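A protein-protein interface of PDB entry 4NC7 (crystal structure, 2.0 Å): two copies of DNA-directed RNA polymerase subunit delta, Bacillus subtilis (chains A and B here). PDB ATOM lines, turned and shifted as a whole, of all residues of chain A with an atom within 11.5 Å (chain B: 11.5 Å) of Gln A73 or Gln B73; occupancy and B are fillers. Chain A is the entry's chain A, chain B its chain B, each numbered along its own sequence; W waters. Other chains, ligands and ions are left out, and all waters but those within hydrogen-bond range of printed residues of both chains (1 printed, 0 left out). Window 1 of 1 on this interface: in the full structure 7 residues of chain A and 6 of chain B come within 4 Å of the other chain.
Water W1 lies within hydrogen-bond range of OE1 of Gln A73 (2.9 Å) and OE1 of Gln B73 (3.2 Å).
Among the printed residues, merely in contact across the chains: Ala A69 with Ala B69 (3.3 Å), Tyr A58 with Leu B70 (3.6 Å) and Leu A70 with Tyr B58 (3.8 Å).
Val A30 touches none of the printed residues of chain B.
Printed residues of chain B within 4 Å of Ala A69: Tyr B58 (2.8 Å) and Ala B69 (3.3 Å).
Of the printed residues of chain B, Ser A71 touches Tyr B58.
Printed residues of chain B within 4 Å of Gln A73: Gln B73.
Glu B34 touches none of the printed residues of chain A.
Of the printed residues of chain A, Tyr B58 touches Ala A69 (2.8 Å), Leu A70 (3.8 Å) and Ser A71 (3.4 Å).
Of the printed residues of chain A, Ala B69 touches Tyr A58 and Ala A69.
Printed residues of chain A within 4 Å of Leu B70: Tyr A58 (3.6 Å).
No residue of chain A comes within 4 Å of Ser B71.
Of the printed residues of chain A, Gln B73 touches Gln A73 (2.8 Å).
No residue of chain A comes within 4 Å of Trp B75.
The nearest printed residue of chain A that does not touch Tyr B58 is Asp A72 (6.7 Å).
Of the 17 printed residues of chain A, 5 touch a printed residue of chain B.
Hydrophobic or aromatic side chains of chain A within 4 Å of the printed part of chain B: Tyr A58 and Ala A69.
Among the printed residues, no Asp or Glu carboxylate lies within 4 Å of a Lys or Arg side-chain nitrogen of the other chain.
OH of Tyr A58 lies within hydrogen-bond range of O of Ala B69 (2.7 Å).
The backbone carbonyl oxygen (O) of Ala A69 lies within hydrogen-bond range of the side-chain hydroxyl (OH) of Tyr B58, 2.8 Å away.
The side-chain hydroxyl (OG) of Ser A71 is in hydrogen-bond range of the side-chain hydroxyl (OH) of Tyr B58, 3.4 Å away.
NE2 of Gln A73 sits at hydrogen-bond distance from OE1 of Gln B73 (2.8 Å).
Tyr A58 touches Ala B69, and with the chains exchanged Ala A69 touches Tyr B58.
Ala B69 touches its own counterpart, Ala A69.
Ser A71 touches Tyr B58, but with the chains exchanged Tyr A58 does not touch Ser B71 (4.9 Å).
Gln B73 touches its own counterpart, Gln A73.
Positions printed for both chains: 29, 30, 31, 32, 58, 69, 70, 71, 72, 73, 74, 75, 76, 77, 80 and 81.
Of the 7 pairs that touch across the chains among the printed residues, 6 have their exchanged pair printed and touching as well.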
ATOM      1  N   PRO A  29      -6.170 -16.140 -22.082  1.00  0.00           N
ATOM      2  CA  PRO A  29      -5.952 -16.634 -20.694  1.00  0.00           C
ATOM      3  C   PRO A  29      -5.858 -18.126 -20.603  1.00  0.00           C
ATOM      4  O   PRO A  29      -6.554 -18.799 -21.332  1.00  0.00           O
ATOM      5  CB  PRO A  29      -7.202 -16.127 -19.953  1.00  0.00           C
ATOM      6  CG  PRO A  29      -7.562 -14.855 -20.719  1.00  0.00           C
ATOM      7  CD  PRO A  29      -7.392 -15.331 -22.162  1.00  0.00           C
ATOM      8  N   VAL A  30      -5.035 -18.664 -19.679  1.00  0.00           N
ATOM      9  CA  VAL A  30      -4.816 -20.095 -19.563  1.00  0.00           C
ATOM     10  C   VAL A  30      -4.772 -20.376 -18.055  1.00  0.00           C
ATOM     11  O   VAL A  30      -4.086 -19.657 -17.310  1.00  0.00           O
ATOM     12  CB  VAL A  30      -3.445 -20.512 -20.172  1.00  0.00           C
ATOM     13  CG1 VAL A  30      -3.299 -22.038 -20.168  1.00  0.00           C
ATOM     14  CG2 VAL A  30      -3.244 -19.909 -21.563  1.00  0.00           C
ATOM     15  N   PRO A  31      -5.531 -21.359 -17.600  1.00  0.00           N
ATOM     16  CA  PRO A  31      -5.468 -21.704 -16.217  1.00  0.00           C
ATOM     17  C   PRO A  31      -4.162 -22.385 -15.876  1.00  0.00           C
ATOM     18  O   PRO A  31      -3.583 -23.060 -16.745  1.00  0.00           O
ATOM     19  CB  PRO A  31      -6.539 -22.718 -16.038  1.00  0.00           C
ATOM     20  CG  PRO A  31      -7.376 -22.678 -17.196  1.00  0.00           C
ATOM     21  CD  PRO A  31      -6.523 -22.177 -18.308  1.00  0.00           C
ATOM     22  N   PHE A  32      -3.763 -22.257 -14.630  1.00  0.00           N
ATOM     23  CA  PHE A  32      -2.462 -22.747 -14.135  1.00  0.00           C
ATOM     24  C   PHE A  32      -2.197 -24.222 -14.423  1.00  0.00           C
ATOM     25  O   PHE A  32      -1.116 -24.598 -14.894  1.00  0.00           O
ATOM     26  CB  PHE A  32      -2.363 -22.496 -12.640  1.00  0.00           C
ATOM     27  CG  PHE A  32      -0.945 -22.662 -12.078  1.00  0.00           C
ATOM     28  CD1 PHE A  32       0.056 -21.762 -12.410  1.00  0.00           C
ATOM     29  CD2 PHE A  32      -0.652 -23.660 -11.167  1.00  0.00           C
ATOM     30  CE1 PHE A  32       1.330 -21.853 -11.867  1.00  0.00           C
ATOM     31  CE2 PHE A  32       0.650 -23.765 -10.615  1.00  0.00           C
ATOM     32  CZ  PHE A  32       1.620 -22.863 -10.995  1.00  0.00           C
ATOM     33  N   GLN A  33      -3.168 -25.087 -14.153  1.00  0.00           N
ATOM     34  CA  GLN A  33      -2.965 -26.518 -14.453  1.00  0.00           C
ATOM     35  C   GLN A  33      -2.778 -26.826 -15.922  1.00  0.00           C
ATOM     36  O   GLN A  33      -2.000 -27.718 -16.274  1.00  0.00           O
ATOM     37  CB  GLN A  33      -4.058 -27.405 -13.861  1.00  0.00           C
ATOM     38  CG  GLN A  33      -4.137 -27.377 -12.343  1.00  0.00           C
ATOM     39  CD  GLN A  33      -2.855 -27.809 -11.610  1.00  0.00           C
ATOM     40  OE1 GLN A  33      -2.471 -27.228 -10.592  1.00  0.00           O
ATOM     41  NE2 GLN A  33      -2.189 -28.789 -12.131  1.00  0.00           N
ATOM     42  N   TYR A  58       4.747 -19.993  -9.684  1.00  0.00           N
ATOM     43  CA  TYR A  58       3.617 -19.302  -9.146  1.00  0.00           C
ATOM     44  C   TYR A  58       4.063 -17.927  -8.603  1.00  0.00           C
ATOM     45  O   TYR A  58       3.437 -16.889  -8.891  1.00  0.00           O
ATOM     46  CB  TYR A  58       3.020 -20.210  -8.089  1.00  0.00           C
ATOM     47  CG  TYR A  58       2.023 -19.509  -7.219  1.00  0.00           C
ATOM     48  CD1 TYR A  58       0.701 -19.326  -7.650  1.00  0.00           C
ATOM     49  CD2 TYR A  58       2.411 -18.981  -5.967  1.00  0.00           C
ATOM     50  CE1 TYR A  58      -0.239 -18.668  -6.851  1.00  0.00           C
ATOM     51  CE2 TYR A  58       1.487 -18.285  -5.161  1.00  0.00           C
ATOM     52  CZ  TYR A  58       0.165 -18.120  -5.607  1.00  0.00           C
ATOM     53  OH  TYR A  58      -0.745 -17.430  -4.777  1.00  0.00           O
ATOM     54  N   ALA A  69      -3.442 -12.346 -12.714  1.00  0.00           N
ATOM     55  CA  ALA A  69      -4.357 -13.369 -12.225  1.00  0.00           C
ATOM     56  C   ALA A  69      -5.769 -12.849 -12.547  1.00  0.00           C
ATOM     57  O   ALA A  69      -6.169 -11.755 -12.119  1.00  0.00           O
ATOM     58  CB  ALA A  69      -4.179 -13.556 -10.768  1.00  0.00           C
ATOM     59  N   LEU A  70      -6.469 -13.598 -13.394  1.00  0.00           N
ATOM     60  CA  LEU A  70      -7.814 -13.283 -13.823  1.00  0.00           C
ATOM     61  C   LEU A  70      -8.831 -14.142 -13.038  1.00  0.00           C
ATOM     62  O   LEU A  70      -8.529 -15.275 -12.546  1.00  0.00           O
ATOM     63  CB  LEU A  70      -7.958 -13.493 -15.339  1.00  0.00           C
ATOM     64  CG  LEU A  70      -6.934 -12.683 -16.132  1.00  0.00           C
ATOM     65  CD1 LEU A  70      -6.773 -13.179 -17.561  1.00  0.00           C
ATOM     66  CD2 LEU A  70      -7.272 -11.197 -16.036  1.00  0.00           C
ATOM     67  N   SER A  71     -10.008 -13.567 -12.834  1.00  0.00           N
ATOM     68  CA  SER A  71     -11.083 -14.335 -12.225  1.00  0.00           C
ATOM     69  C   SER A  71     -11.784 -15.110 -13.336  1.00  0.00           C
ATOM     70  O   SER A  71     -12.018 -14.592 -14.416  1.00  0.00           O
ATOM     71  CB  SER A  71     -12.055 -13.425 -11.455  1.00  0.00           C
ATOM     72  OG  SER A  71     -11.373 -12.958 -10.304  1.00  0.00           O
ATOM     73  N   ASP A  72     -11.946 -16.391 -13.138  1.00  0.00           N
ATOM     74  CA  ASP A  72     -12.823 -17.212 -13.997  1.00  0.00           C
ATOM     75  C   ASP A  72     -12.947 -18.462 -13.169  1.00  0.00           C
ATOM     76  O   ASP A  72     -12.037 -18.760 -12.410  1.00  0.00           O
ATOM     77  CB  ASP A  72     -12.176 -17.541 -15.342  1.00  0.00           C
ATOM     78  CG  ASP A  72     -13.197 -18.054 -16.368  1.00  0.00           C
ATOM     79  OD1 ASP A  72     -14.397 -18.042 -16.056  1.00  0.00           O
ATOM     80  OD2 ASP A  72     -12.803 -18.520 -17.427  1.00  0.00           O
ATOM     81  N   GLN A  73     -14.064 -19.162 -13.280  1.00  0.00           N
ATOM     82  CA  GLN A  73     -14.275 -20.404 -12.555  1.00  0.00           C
ATOM     83  C   GLN A  73     -14.029 -21.581 -13.443  1.00  0.00           C
ATOM     84  O   GLN A  73     -14.666 -21.705 -14.489  1.00  0.00           O
ATOM     85  CB  GLN A  73     -15.722 -20.457 -12.067  1.00  0.00           C
ATOM     86  CG  GLN A  73     -16.072 -21.589 -11.147  1.00  0.00           C
ATOM     87  CD  GLN A  73     -15.306 -21.504  -9.854  1.00  0.00           C
ATOM     88  OE1 GLN A  73     -15.349 -20.484  -9.146  1.00  0.00           O
ATOM     89  NE2 GLN A  73     -14.524 -22.509  -9.594  1.00  0.00           N
ATOM     90  N   THR A  74     -13.166 -22.488 -12.988  1.00  0.00           N
ATOM     91  CA  THR A  74     -13.035 -23.795 -13.578  1.00  0.00           C
ATOM     92  C   THR A  74     -14.114 -24.754 -13.080  1.00  0.00           C
ATOM     93  O   THR A  74     -14.421 -24.810 -11.839  1.00  0.00           O
ATOM     94  CB  THR A  74     -11.642 -24.397 -13.325  1.00  0.00           C
ATOM     95  OG1 THR A  74     -10.593 -23.554 -13.885  1.00  0.00           O
ATOM     96  CG2 THR A  74     -11.517 -25.812 -13.867  1.00  0.00           C
ATOM     97  N   TRP A  75     -14.631 -25.539 -14.018  1.00  0.00           N
ATOM     98  CA  TRP A  75     -15.720 -26.492 -13.748  1.00  0.00           C
ATOM     99  C   TRP A  75     -15.305 -27.843 -14.217  1.00  0.00           C
ATOM    100  O   TRP A  75     -14.556 -27.973 -15.216  1.00  0.00           O
ATOM    101  CB  TRP A  75     -17.009 -26.080 -14.455  1.00  0.00           C
ATOM    102  CG  TRP A  75     -17.680 -24.878 -13.847  1.00  0.00           C
ATOM    103  CD1 TRP A  75     -17.562 -23.575 -14.266  1.00  0.00           C
ATOM    104  CD2 TRP A  75     -18.488 -24.843 -12.674  1.00  0.00           C
ATOM    105  NE1 TRP A  75     -18.236 -22.766 -13.442  1.00  0.00           N
ATOM    106  CE2 TRP A  75     -18.831 -23.508 -12.455  1.00  0.00           C
ATOM    107  CE3 TRP A  75     -18.965 -25.825 -11.782  1.00  0.00           C
ATOM    108  CZ2 TRP A  75     -19.623 -23.087 -11.359  1.00  0.00           C
ATOM    109  CZ3 TRP A  75     -19.776 -25.400 -10.697  1.00  0.00           C
ATOM    110  CH2 TRP A  75     -20.110 -24.049 -10.535  1.00  0.00           C
ATOM    111  N   GLY A  76     -15.741 -28.896 -13.511  1.00  0.00           N
ATOM    112  CA  GLY A  76     -15.632 -30.218 -14.100  1.00  0.00           C
ATOM    113  C   GLY A  76     -16.768 -31.114 -13.619  1.00  0.00           C
ATOM    114  O   GLY A  76     -17.679 -30.658 -12.970  1.00  0.00           O
ATOM    115  N   LEU A  77     -16.641 -32.402 -13.870  1.00  0.00           N
ATOM    116  CA  LEU A  77     -17.692 -33.375 -13.561  1.00  0.00           C
ATOM    117  C   LEU A  77     -17.322 -34.090 -12.258  1.00  0.00           C
ATOM    118  O   LEU A  77     -16.192 -34.535 -12.095  1.00  0.00           O
ATOM    119  CB  LEU A  77     -17.803 -34.391 -14.689  1.00  0.00           C
ATOM    120  CG  LEU A  77     -18.386 -33.911 -16.012  1.00  0.00           C
ATOM    121  CD1 LEU A  77     -18.568 -35.129 -16.923  1.00  0.00           C
ATOM    122  CD2 LEU A  77     -19.693 -33.179 -15.820  1.00  0.00           C
ATOM    123  N   TRP A  80     -15.609 -37.533 -12.140  1.00  0.00           N
ATOM    124  CA  TRP A  80     -14.168 -37.707 -12.409  1.00  0.00           C
ATOM    125  C   TRP A  80     -13.226 -37.886 -11.199  1.00  0.00           C
ATOM    126  O   TRP A  80     -12.006 -37.942 -11.391  1.00  0.00           O
ATOM    127  CB  TRP A  80     -13.596 -36.522 -13.203  1.00  0.00           C
ATOM    128  CG  TRP A  80     -14.120 -36.318 -14.596  1.00  0.00           C
ATOM    129  CD1 TRP A  80     -14.696 -37.244 -15.412  1.00  0.00           C
ATOM    130  CD2 TRP A  80     -14.066 -35.097 -15.346  1.00  0.00           C
ATOM    131  NE1 TRP A  80     -15.048 -36.667 -16.598  1.00  0.00           N
ATOM    132  CE2 TRP A  80     -14.645 -35.354 -16.597  1.00  0.00           C
ATOM    133  CE3 TRP A  80     -13.588 -33.816 -15.073  1.00  0.00           C
ATOM    134  CZ2 TRP A  80     -14.770 -34.361 -17.581  1.00  0.00           C
ATOM    135  CZ3 TRP A  80     -13.709 -32.824 -16.056  1.00  0.00           C
ATOM    136  CH2 TRP A  80     -14.298 -33.100 -17.278  1.00  0.00           C
ATOM    137  N   TYR A  81     -13.726 -37.921  -9.971  1.00  0.00           N
ATOM    138  CA  TYR A  81     -12.817 -37.802  -8.828  1.00  0.00           C
ATOM    139  C   TYR A  81     -12.892 -38.924  -7.786  1.00  0.00           C
ATOM    140  O   TYR A  81     -13.868 -39.034  -7.073  1.00  0.00           O
ATOM    141  CB  TYR A  81     -12.979 -36.402  -8.247  1.00  0.00           C
ATOM    142  CG  TYR A  81     -12.450 -35.389  -9.240  1.00  0.00           C
ATOM    143  CD1 TYR A  81     -13.313 -34.558  -9.977  1.00  0.00           C
ATOM    144  CD2 TYR A  81     -11.083 -35.340  -9.527  1.00  0.00           C
ATOM    145  CE1 TYR A  81     -12.817 -33.676 -10.940  1.00  0.00           C
ATOM    146  CE2 TYR A  81     -10.584 -34.462 -10.473  1.00  0.00           C
ATOM    147  CZ  TYR A  81     -11.444 -33.635 -11.170  1.00  0.00           C
ATOM    148  OH  TYR A  81     -10.898 -32.773 -12.088  1.00  0.00           O
ATOM    149  N   PRO B  29      -6.651 -13.807   4.044  1.00  0.00           N
ATOM    150  CA  PRO B  29      -7.107 -13.577   2.671  1.00  0.00           C
ATOM    151  C   PRO B  29      -8.549 -13.143   2.589  1.00  0.00           C
ATOM    152  O   PRO B  29      -9.378 -13.580   3.401  1.00  0.00           O
ATOM    153  CB  PRO B  29      -6.929 -14.923   2.002  1.00  0.00           C
ATOM    154  CG  PRO B  29      -5.974 -15.706   2.873  1.00  0.00           C
ATOM    155  CD  PRO B  29      -6.166 -15.173   4.257  1.00  0.00           C
ATOM    156  N   VAL B  30      -8.816 -12.299   1.592  1.00  0.00           N
ATOM    157  CA  VAL B  30     -10.098 -11.667   1.356  1.00  0.00           C
ATOM    158  C   VAL B  30     -10.408 -11.824  -0.103  1.00  0.00           C
ATOM    159  O   VAL B  30      -9.560 -11.489  -0.927  1.00  0.00           O
ATOM    160  CB  VAL B  30      -9.957 -10.124   1.628  1.00  0.00           C
ATOM    161  CG1 VAL B  30     -11.216  -9.360   1.314  1.00  0.00           C
ATOM    162  CG2 VAL B  30      -9.582  -9.870   3.072  1.00  0.00           C
ATOM    163  N   PRO B  31     -11.666 -12.139  -0.444  1.00  0.00           N
ATOM    164  CA  PRO B  31     -12.100 -11.934  -1.825  1.00  0.00           C
ATOM    165  C   PRO B  31     -12.045 -10.482  -2.255  1.00  0.00           C
ATOM    166  O   PRO B  31     -12.296  -9.598  -1.430  1.00  0.00           O
ATOM    167  CB  PRO B  31     -13.548 -12.427  -1.820  1.00  0.00           C
ATOM    168  CG  PRO B  31     -13.675 -13.198  -0.569  1.00  0.00           C
ATOM    169  CD  PRO B  31     -12.763 -12.640   0.408  1.00  0.00           C
ATOM    170  N   PHE B  32     -11.770 -10.232  -3.544  1.00  0.00           N
ATOM    171  CA  PHE B  32     -11.658  -8.873  -4.101  1.00  0.00           C
ATOM    172  C   PHE B  32     -12.873  -7.960  -3.799  1.00  0.00           C
ATOM    173  O   PHE B  32     -12.701  -6.805  -3.413  1.00  0.00           O
ATOM    174  CB  PHE B  32     -11.468  -8.937  -5.637  1.00  0.00           C
ATOM    175  CG  PHE B  32     -11.212  -7.590  -6.287  1.00  0.00           C
ATOM    176  CD1 PHE B  32     -10.028  -6.899  -6.036  1.00  0.00           C
ATOM    177  CD2 PHE B  32     -12.158  -7.007  -7.128  1.00  0.00           C
ATOM    178  CE1 PHE B  32      -9.802  -5.659  -6.633  1.00  0.00           C
ATOM    179  CE2 PHE B  32     -11.926  -5.769  -7.710  1.00  0.00           C
ATOM    180  CZ  PHE B  32     -10.748  -5.114  -7.475  1.00  0.00           C
ATOM    181  N   GLU B  34     -14.919  -8.174  -1.342  1.00  0.00           N
ATOM    182  CA  GLU B  34     -15.014  -7.834   0.072  1.00  0.00           C
ATOM    183  C   GLU B  34     -13.991  -6.736   0.382  1.00  0.00           C
ATOM    184  O   GLU B  34     -14.263  -5.804   1.138  1.00  0.00           O
ATOM    185  CB  GLU B  34     -14.852  -9.064   0.975  1.00  0.00           C
ATOM    186  CG  GLU B  34     -16.153  -9.918   1.121  1.00  0.00           C
ATOM    187  CD  GLU B  34     -17.465  -9.089   1.312  1.00  0.00           C
ATOM    188  OE1 GLU B  34     -17.589  -8.364   2.336  1.00  0.00           O
ATOM    189  OE2 GLU B  34     -18.376  -9.141   0.428  1.00  0.00           O
ATOM    190  N   TYR B  58      -7.370  -3.368  -9.180  1.00  0.00           N
ATOM    191  CA  TYR B  58      -7.051  -4.811  -9.526  1.00  0.00           C
ATOM    192  C   TYR B  58      -5.674  -4.882 -10.269  1.00  0.00           C
ATOM    193  O   TYR B  58      -4.887  -5.806 -10.032  1.00  0.00           O
ATOM    194  CB  TYR B  58      -8.210  -5.568 -10.299  1.00  0.00           C
ATOM    195  CG  TYR B  58      -8.241  -7.164 -10.273  1.00  0.00           C
ATOM    196  CD1 TYR B  58      -9.007  -7.901  -9.335  1.00  0.00           C
ATOM    197  CD2 TYR B  58      -7.539  -7.919 -11.213  1.00  0.00           C
ATOM    198  CE1 TYR B  58      -9.032  -9.337  -9.314  1.00  0.00           C
ATOM    199  CE2 TYR B  58      -7.571  -9.323 -11.212  1.00  0.00           C
ATOM    200  CZ  TYR B  58      -8.311 -10.051 -10.285  1.00  0.00           C
ATOM    201  OH  TYR B  58      -8.287 -11.495 -10.345  1.00  0.00           O
ATOM    202  N   ALA B  69      -2.140 -13.446  -5.669  1.00  0.00           N
ATOM    203  CA  ALA B  69      -3.441 -13.915  -6.074  1.00  0.00           C
ATOM    204  C   ALA B  69      -3.522 -15.357  -5.649  1.00  0.00           C
ATOM    205  O   ALA B  69      -2.688 -16.194  -6.112  1.00  0.00           O
ATOM    206  CB  ALA B  69      -3.583 -13.819  -7.553  1.00  0.00           C
ATOM    207  N   LEU B  70      -4.470 -15.664  -4.768  1.00  0.00           N
ATOM    208  CA  LEU B  70      -4.528 -17.028  -4.167  1.00  0.00           C
ATOM    209  C   LEU B  70      -5.560 -17.848  -4.903  1.00  0.00           C
ATOM    210  O   LEU B  70      -6.595 -17.302  -5.345  1.00  0.00           O
ATOM    211  CB  LEU B  70      -4.861 -16.954  -2.686  1.00  0.00           C
ATOM    212  CG  LEU B  70      -3.765 -16.179  -1.924  1.00  0.00           C
ATOM    213  CD1 LEU B  70      -4.324 -15.765  -0.602  1.00  0.00           C
ATOM    214  CD2 LEU B  70      -2.530 -17.065  -1.716  1.00  0.00           C
ATOM    215  N   SER B  71      -5.323 -19.142  -5.070  1.00  0.00           N
ATOM    216  CA  SER B  71      -6.224 -19.907  -5.920  1.00  0.00           C
ATOM    217  C   SER B  71      -7.464 -20.409  -5.143  1.00  0.00           C
ATOM    218  O   SER B  71      -8.445 -20.867  -5.737  1.00  0.00           O
ATOM    219  CB  SER B  71      -5.502 -21.040  -6.675  1.00  0.00           C
ATOM    220  OG  SER B  71      -5.097 -22.042  -5.759  1.00  0.00           O
ATOM    221  N   ASP B  72      -7.479 -20.183  -3.843  1.00  0.00           N
ATOM    222  CA  ASP B  72      -8.561 -20.633  -3.027  1.00  0.00           C
ATOM    223  C   ASP B  72      -9.985 -20.242  -3.576  1.00  0.00           C
ATOM    224  O   ASP B  72     -10.215 -19.174  -4.141  1.00  0.00           O
ATOM    225  CB  ASP B  72      -8.371 -20.154  -1.611  1.00  0.00           C
ATOM    226  CG  ASP B  72      -9.178 -20.979  -0.615  1.00  0.00           C
ATOM    227  OD1 ASP B  72      -9.570 -22.141  -0.950  1.00  0.00           O
ATOM    228  OD2 ASP B  72      -9.431 -20.453   0.482  1.00  0.00           O
ATOM    229  N   GLN B  73     -10.912 -21.153  -3.405  1.00  0.00           N
ATOM    230  CA  GLN B  73     -12.342 -21.014  -3.864  1.00  0.00           C
ATOM    231  C   GLN B  73     -13.174 -20.166  -2.893  1.00  0.00           C
ATOM    232  O   GLN B  73     -13.210 -20.474  -1.694  1.00  0.00           O
ATOM    233  CB  GLN B  73     -12.965 -22.402  -4.066  1.00  0.00           C
ATOM    234  CG  GLN B  73     -14.398 -22.359  -4.644  1.00  0.00           C
ATOM    235  CD  GLN B  73     -14.458 -21.821  -6.054  1.00  0.00           C
ATOM    236  OE1 GLN B  73     -13.847 -22.393  -6.923  1.00  0.00           O
ATOM    237  NE2 GLN B  73     -15.253 -20.763  -6.300  1.00  0.00           N
ATOM    238  N   THR B  74     -13.799 -19.101  -3.405  1.00  0.00           N
ATOM    239  CA  THR B  74     -14.787 -18.246  -2.649  1.00  0.00           C
ATOM    240  C   THR B  74     -16.106 -18.942  -2.706  1.00  0.00           C
ATOM    241  O   THR B  74     -16.434 -19.437  -3.732  1.00  0.00           O
ATOM    242  CB  THR B  74     -14.882 -16.825  -3.200  1.00  0.00           C
ATOM    243  OG1 THR B  74     -13.596 -16.226  -3.074  1.00  0.00           O
ATOM    244  CG2 THR B  74     -15.934 -15.905  -2.412  1.00  0.00           C
ATOM    245  N   TRP B  75     -16.762 -19.086  -1.559  1.00  0.00           N
ATOM    246  CA  TRP B  75     -18.072 -19.743  -1.422  1.00  0.00           C
ATOM    247  C   TRP B  75     -19.000 -18.775  -0.796  1.00  0.00           C
ATOM    248  O   TRP B  75     -18.556 -17.922  -0.052  1.00  0.00           O
ATOM    249  CB  TRP B  75     -17.978 -20.952  -0.500  1.00  0.00           C
ATOM    250  CG  TRP B  75     -17.303 -22.100  -1.167  1.00  0.00           C
ATOM    251  CD1 TRP B  75     -16.016 -22.501  -1.016  1.00  0.00           C
ATOM    252  CD2 TRP B  75     -17.905 -23.003  -2.076  1.00  0.00           C
ATOM    253  NE1 TRP B  75     -15.781 -23.620  -1.783  1.00  0.00           N
ATOM    254  CE2 TRP B  75     -16.916 -23.901  -2.490  1.00  0.00           C
ATOM    255  CE3 TRP B  75     -19.191 -23.106  -2.629  1.00  0.00           C
ATOM    256  CZ2 TRP B  75     -17.180 -24.940  -3.389  1.00  0.00           C
ATOM    257  CZ3 TRP B  75     -19.434 -24.076  -3.534  1.00  0.00           C
ATOM    258  CH2 TRP B  75     -18.443 -25.008  -3.892  1.00  0.00           C
ATOM    259  N   GLY B  76     -20.289 -18.907  -1.059  1.00  0.00           N
ATOM    260  CA  GLY B  76     -21.299 -18.005  -0.476  1.00  0.00           C
ATOM    261  C   GLY B  76     -22.664 -18.664  -0.603  1.00  0.00           C
ATOM    262  O   GLY B  76     -22.755 -19.810  -1.076  1.00  0.00           O
ATOM    263  N   LEU B  77     -23.735 -17.981  -0.181  1.00  0.00           N
ATOM    264  CA  LEU B  77     -25.080 -18.612  -0.195  1.00  0.00           C
ATOM    265  C   LEU B  77     -25.865 -18.078  -1.393  1.00  0.00           C
ATOM    266  O   LEU B  77     -25.863 -16.883  -1.680  1.00  0.00           O
ATOM    267  CB  LEU B  77     -25.887 -18.432   1.097  1.00  0.00           C
ATOM    268  CG  LEU B  77     -25.348 -18.864   2.473  1.00  0.00           C
ATOM    269  CD1 LEU B  77     -26.366 -18.562   3.568  1.00  0.00           C
ATOM    270  CD2 LEU B  77     -24.995 -20.309   2.491  1.00  0.00           C
ATOM    271  N   TRP B  80     -28.195 -15.025  -1.265  1.00  0.00           N
ATOM    272  CA  TRP B  80     -27.689 -13.654  -1.296  1.00  0.00           C
ATOM    273  C   TRP B  80     -27.776 -12.974  -2.670  1.00  0.00           C
ATOM    274  O   TRP B  80     -27.312 -11.841  -2.807  1.00  0.00           O
ATOM    275  CB  TRP B  80     -26.241 -13.625  -0.805  1.00  0.00           C
ATOM    276  CG  TRP B  80     -26.042 -14.167   0.564  1.00  0.00           C
ATOM    277  CD1 TRP B  80     -26.997 -14.350   1.530  1.00  0.00           C
ATOM    278  CD2 TRP B  80     -24.794 -14.547   1.155  1.00  0.00           C
ATOM    279  NE1 TRP B  80     -26.423 -14.863   2.658  1.00  0.00           N
ATOM    280  CE2 TRP B  80     -25.070 -14.975   2.468  1.00  0.00           C
ATOM    281  CE3 TRP B  80     -23.471 -14.577   0.694  1.00  0.00           C
ATOM    282  CZ2 TRP B  80     -24.073 -15.437   3.324  1.00  0.00           C
ATOM    283  CZ3 TRP B  80     -22.498 -15.064   1.520  1.00  0.00           C
ATOM    284  CH2 TRP B  80     -22.791 -15.465   2.831  1.00  0.00           C
ATOM    285  N   TYR B  81     -28.329 -13.656  -3.681  1.00  0.00           N
ATOM    286  CA  TYR B  81     -28.337 -13.146  -5.065  1.00  0.00           C
ATOM    287  C   TYR B  81     -29.644 -13.451  -5.805  1.00  0.00           C
ATOM    288  O   TYR B  81     -29.936 -12.841  -6.844  1.00  0.00           O
ATOM    289  CB  TYR B  81     -27.131 -13.715  -5.846  1.00  0.00           C
ATOM    290  CG  TYR B  81     -25.791 -13.621  -5.104  1.00  0.00           C
ATOM    291  CD1 TYR B  81     -25.046 -12.432  -5.082  1.00  0.00           C
ATOM    292  CD2 TYR B  81     -25.273 -14.718  -4.416  1.00  0.00           C
ATOM    293  CE1 TYR B  81     -23.837 -12.361  -4.408  1.00  0.00           C
ATOM    294  CE2 TYR B  81     -24.073 -14.648  -3.757  1.00  0.00           C
ATOM    295  CZ  TYR B  81     -23.364 -13.479  -3.755  1.00  0.00           C
ATOM    296  OH  TYR B  81     -22.194 -13.435  -3.058  1.00  0.00           O
HETATM  297  O   HOH W   1     -12.618 -19.859  -8.412  1.00  0.00           O
